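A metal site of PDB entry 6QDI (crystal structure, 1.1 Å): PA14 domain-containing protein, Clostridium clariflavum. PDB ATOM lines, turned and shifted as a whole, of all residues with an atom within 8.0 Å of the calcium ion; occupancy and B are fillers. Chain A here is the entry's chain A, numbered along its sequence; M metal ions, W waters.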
ATOM      1  N   PHE A 162      -5.016  13.506  18.076  1.00  0.00           N
ATOM      2  CA  PHE A 162      -3.629  13.363  17.638  1.00  0.00           C
ATOM      3  C   PHE A 162      -3.327  14.234  16.443  1.00  0.00           C
ATOM      4  O   PHE A 162      -4.136  14.349  15.503  1.00  0.00           O
ATOM      5  CB  PHE A 162      -3.396  11.900  17.249  1.00  0.00           C
ATOM      6  CG  PHE A 162      -3.552  10.936  18.417  1.00  0.00           C
ATOM      7  CD1 PHE A 162      -2.482  10.699  19.282  1.00  0.00           C
ATOM      8  CD2 PHE A 162      -4.734  10.266  18.621  1.00  0.00           C
ATOM      9  CE1 PHE A 162      -2.612   9.799  20.340  1.00  0.00           C
ATOM     10  CE2 PHE A 162      -4.864   9.362  19.665  1.00  0.00           C
ATOM     11  CZ  PHE A 162      -3.803   9.140  20.525  1.00  0.00           C
ATOM     12  N   ASP A 163      -2.135  14.852  16.475  1.00  0.00           N
ATOM     13  CA  ASP A 163      -1.734  15.765  15.410  1.00  0.00           C
ATOM     14  C   ASP A 163      -1.228  15.063  14.169  1.00  0.00           C
ATOM     15  O   ASP A 163      -1.155  15.674  13.102  1.00  0.00           O
ATOM     16  CB  ASP A 163      -0.648  16.718  15.930  1.00  0.00           C
ATOM     17  CG  ASP A 163      -0.935  18.198  15.743  1.00  0.00           C
ATOM     18  OD1 ASP A 163      -2.003  18.571  15.246  1.00  0.00           O
ATOM     19  OD2 ASP A 163      -0.067  19.004  16.171  1.00  0.00           O
ATOM     20  N   GLU A 164      -0.852  13.804  14.276  1.00  0.00           N
ATOM     21  CA  GLU A 164      -0.529  12.986  13.107  1.00  0.00           C
ATOM     22  C   GLU A 164      -1.720  12.101  12.779  1.00  0.00           C
ATOM     23  O   GLU A 164      -2.571  11.846  13.647  1.00  0.00           O
ATOM     24  CB  GLU A 164       0.702  12.111  13.379  1.00  0.00           C
ATOM     25  CG  GLU A 164       1.963  12.917  13.588  1.00  0.00           C
ATOM     26  CD  GLU A 164       2.574  13.406  12.296  1.00  0.00           C
ATOM     27  OE1 GLU A 164       2.497  12.745  11.230  1.00  0.00           O
ATOM     28  OE2 GLU A 164       3.192  14.487  12.362  1.00  0.00           O
ATOM     29  N   ASP A 165      -1.764  11.601  11.556  1.00  0.00           N
ATOM     30  CA  ASP A 165      -2.870  10.755  11.072  1.00  0.00           C
ATOM     31  C   ASP A 165      -2.802   9.309  11.530  1.00  0.00           C
ATOM     32  O   ASP A 165      -3.646   8.523  11.135  1.00  0.00           O
ATOM     33  CB  ASP A 165      -3.051  10.934   9.566  1.00  0.00           C
ATOM     34  CG  ASP A 165      -2.004  10.290   8.758  1.00  0.00           C
ATOM     35  OD1 ASP A 165      -1.338   9.358   9.255  1.00  0.00           O
ATOM     36  OD2 ASP A 165      -1.859  10.651   7.566  1.00  0.00           O
ATOM     37  N   THR A 168      -0.558   9.268  16.690  1.00  0.00           N
ATOM     38  CA  THR A 168       0.645   9.749  17.428  1.00  0.00           C
ATOM     39  C   THR A 168       0.628  11.279  17.496  1.00  0.00           C
ATOM     40  O   THR A 168      -0.147  11.959  16.806  1.00  0.00           O
ATOM     41  CB  THR A 168       1.970   9.257  16.805  1.00  0.00           C
ATOM     42  OG1 THR A 168       2.182   9.908  15.542  1.00  0.00           O
ATOM     43  CG2 THR A 168       1.943   7.752  16.660  1.00  0.00           C
ATOM     44  N   ASN A 169       1.478  11.803  18.379  1.00  0.00           N
ATOM     45  CA  ASN A 169       1.545  13.234  18.674  1.00  0.00           C
ATOM     46  C   ASN A 169       0.263  13.745  19.317  1.00  0.00           C
ATOM     47  O   ASN A 169      -0.422  14.631  18.779  1.00  0.00           O
ATOM     48  CB  ASN A 169       1.969  14.071  17.463  1.00  0.00           C
ATOM     49  CG  ASN A 169       2.601  15.398  17.861  1.00  0.00           C
ATOM     50  OD1 ASN A 169       2.855  15.660  19.036  1.00  0.00           O
ATOM     51  ND2 ASN A 169       2.830  16.271  16.879  1.00  0.00           N
ATOM     52  N   SER A 187      -9.926  20.955  11.911  1.00  0.00           N
ATOM     53  CA  SER A 187      -9.455  19.929  12.847  1.00  0.00           C
ATOM     54  C   SER A 187     -10.387  19.826  14.034  1.00  0.00           C
ATOM     55  O   SER A 187     -11.281  20.653  14.219  1.00  0.00           O
ATOM     56  CB  SER A 187      -8.032  20.269  13.291  1.00  0.00           C
ATOM     57  OG  SER A 187      -7.200  20.228  12.163  1.00  0.00           O
ATOM     58  N   ILE A 192      -5.061  21.104  17.421  1.00  0.00           N
ATOM     59  CA  ILE A 192      -4.671  20.217  16.321  1.00  0.00           C
ATOM     60  C   ILE A 192      -4.427  21.061  15.090  1.00  0.00           C
ATOM     61  O   ILE A 192      -5.302  21.805  14.638  1.00  0.00           O
ATOM     62  CB  ILE A 192      -5.744  19.133  16.087  1.00  0.00           C
ATOM     63  CG1 ILE A 192      -5.929  18.279  17.347  1.00  0.00           C
ATOM     64  CG2 ILE A 192      -5.455  18.288  14.877  1.00  0.00           C
ATOM     65  CD1 ILE A 192      -4.778  17.311  17.643  1.00  0.00           C
ATOM     66  N   ASN A 193      -3.227  20.977  14.545  1.00  0.00           N
ATOM     67  CA  ASN A 193      -2.855  21.746  13.377  1.00  0.00           C
ATOM     68  C   ASN A 193      -3.864  21.523  12.229  1.00  0.00           C
ATOM     69  O   ASN A 193      -4.311  20.394  11.987  1.00  0.00           O
ATOM     70  CB  ASN A 193      -1.465  21.385  12.917  1.00  0.00           C
ATOM     71  CG  ASN A 193      -0.923  22.370  11.906  1.00  0.00           C
ATOM     72  OD1 ASN A 193      -0.894  23.569  12.133  1.00  0.00           O
ATOM     73  ND2 ASN A 193      -0.574  21.875  10.785  1.00  0.00           N
ATOM     74  N   GLN A 194      -4.197  22.609  11.532  1.00  0.00           N
ATOM     75  CA  GLN A 194      -5.250  22.587  10.496  1.00  0.00           C
ATOM     76  C   GLN A 194      -4.657  22.198   9.135  1.00  0.00           C
ATOM     77  O   GLN A 194      -4.550  23.001   8.197  1.00  0.00           O
ATOM     78  CB  GLN A 194      -5.962  23.901  10.473  1.00  0.00           C
ATOM     79  CG  GLN A 194      -7.302  23.856   9.812  1.00  0.00           C
ATOM     80  CD  GLN A 194      -7.938  25.224   9.826  1.00  0.00           C
ATOM     81  OE1 GLN A 194      -7.629  26.042   8.955  1.00  0.00           O
ATOM     82  NE2 GLN A 194      -8.752  25.518  10.830  1.00  0.00           N
ATOM     83  N   ASP A 195      -4.183  20.931   9.048  1.00  0.00           N
ATOM     84  CA  ASP A 195      -3.511  20.380   7.864  1.00  0.00           C
ATOM     85  C   ASP A 195      -4.204  19.167   7.260  1.00  0.00           C
ATOM     86  O   ASP A 195      -3.633  18.512   6.409  1.00  0.00           O
ATOM     87  CB  ASP A 195      -2.013  20.043   8.179  1.00  0.00           C
ATOM     88  CG  ASP A 195      -1.845  18.976   9.230  1.00  0.00           C
ATOM     89  OD1 ASP A 195      -2.815  18.357   9.632  1.00  0.00           O
ATOM     90  OD2 ASP A 195      -0.686  18.803   9.704  1.00  0.00           O
ATOM     91  N   GLN A 196      -5.425  18.863   7.723  1.00  0.00           N
ATOM     92  CA  GLN A 196      -6.221  17.757   7.190  1.00  0.00           C
ATOM     93  C   GLN A 196      -5.581  16.394   7.358  1.00  0.00           C
ATOM     94  O   GLN A 196      -5.976  15.469   6.729  1.00  0.00           O
ATOM     95  CB  GLN A 196      -6.695  17.965   5.737  1.00  0.00           C
ATOM     96  CG  GLN A 196      -7.480  19.269   5.519  1.00  0.00           C
ATOM     97  CD  GLN A 196      -6.571  20.475   5.425  1.00  0.00           C
ATOM     98  OE1 GLN A 196      -5.611  20.491   4.654  1.00  0.00           O
ATOM     99  NE2 GLN A 196      -6.923  21.523   6.119  1.00  0.00           N
ATOM    100  N   LYS A 197      -4.611  16.280   8.269  1.00  0.00           N
ATOM    101  CA  LYS A 197      -3.924  15.037   8.513  1.00  0.00           C
ATOM    102  C   LYS A 197      -3.866  14.880  10.023  1.00  0.00           C
ATOM    103  O   LYS A 197      -2.969  15.438  10.703  1.00  0.00           O
ATOM    104  CB  LYS A 197      -2.518  15.096   7.920  1.00  0.00           C
ATOM    105  CG  LYS A 197      -2.517  15.151   6.421  1.00  0.00           C
ATOM    106  CD  LYS A 197      -1.104  15.252   5.877  1.00  0.00           C
ATOM    107  CE  LYS A 197      -0.544  16.639   6.098  1.00  0.00           C
ATOM    108  N   PHE A 198      -4.832  14.138  10.582  1.00  0.00           N
ATOM    109  CA  PHE A 198      -4.973  14.055  12.031  1.00  0.00           C
ATOM    110  C   PHE A 198      -5.772  12.800  12.325  1.00  0.00           C
ATOM    111  O   PHE A 198      -6.315  12.181  11.423  1.00  0.00           O
ATOM    112  CB  PHE A 198      -5.601  15.323  12.610  1.00  0.00           C
ATOM    113  CG  PHE A 198      -6.982  15.618  12.096  1.00  0.00           C
ATOM    114  CD1 PHE A 198      -8.099  14.975  12.601  1.00  0.00           C
ATOM    115  CD2 PHE A 198      -7.190  16.568  11.088  1.00  0.00           C
ATOM    116  CE1 PHE A 198      -9.379  15.246  12.074  1.00  0.00           C
ATOM    117  CE2 PHE A 198      -8.459  16.834  10.615  1.00  0.00           C
ATOM    118  CZ  PHE A 198      -9.547  16.196  11.099  1.00  0.00           C
ATOM    119  N   SER A 199      -5.818  12.429  13.618  1.00  0.00           N
ATOM    120  CA  SER A 199      -6.531  11.207  13.977  1.00  0.00           C
ATOM    121  C   SER A 199      -7.076  11.316  15.387  1.00  0.00           C
ATOM    122  O   SER A 199      -6.709  12.217  16.146  1.00  0.00           O
ATOM    123  CB  SER A 199      -5.637   9.985  13.779  1.00  0.00           C
ATOM    124  OG  SER A 199      -4.426  10.090  14.501  1.00  0.00           O
ATOM    125  N   ASN A 266      -8.234  11.473   9.302  1.00  0.00           N
ATOM    126  CA  ASN A 266      -8.272  12.236   8.044  1.00  0.00           C
ATOM    127  C   ASN A 266      -6.846  12.223   7.517  1.00  0.00           C
ATOM    128  O   ASN A 266      -5.914  12.544   8.249  1.00  0.00           O
ATOM    129  CB  ASN A 266      -8.729  13.669   8.257  1.00  0.00           C
ATOM    130  CG  ASN A 266      -9.031  14.378   6.937  1.00  0.00           C
ATOM    131  OD1 ASN A 266      -8.957  13.783   5.868  1.00  0.00           O
ATOM    132  ND2 ASN A 266      -9.375  15.651   7.005  1.00  0.00           N
HETATM  133 CA    CA M   1      -1.370  17.032  11.212  1.00  0.00          CA
HETATM  134  O   HOH W   1      -2.857  18.157  12.650  1.00  0.00           O
HETATM  135  O   HOH W   2       0.485  18.044  12.372  1.00  0.00           O
HETATM  136  O   HOH W   3       0.169  15.680  10.061  1.00  0.00           O
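The backbone carbonyl oxygen (O) of Asn 169 lies within hydrogen-bond range of the backbone NH (N) of Asp 163.
ND2 of Asn 193 sits close to OD2 of Asp 195 (3.3 Å).
The side-chain carboxylate of Asp 163 sits at hydrogen-bond distance from the backbone NH of Asn 193, 2.8 Å away.
Water W1 bridges the backbone carbonyl oxygen (O) of Asn 193 (2.7 Å) and the side-chain carboxylate (OD1) of Asp 163 (2.8 Å).
Within 4 Å of the calcium ion: Asp 163, Asp 195 and Lys 197.
Along chain A the residues within 4 Å of the calcium ion span positions 163 to 197.
The nearest printed residue that does not touch the calcium ion is Glu 164 (4.5 Å).
The calcium ion is bound by the backbone carbonyl oxygen (O) of Lys 197, the backbone carbonyl oxygen (O) of Asp 163, water W3, water W1, water W2, the side-chain carboxylate (OD2) of Asp 195 and the side-chain carboxylate (OD1) of Asp 195.
The calcium ion has seven donor atoms within binding distance.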
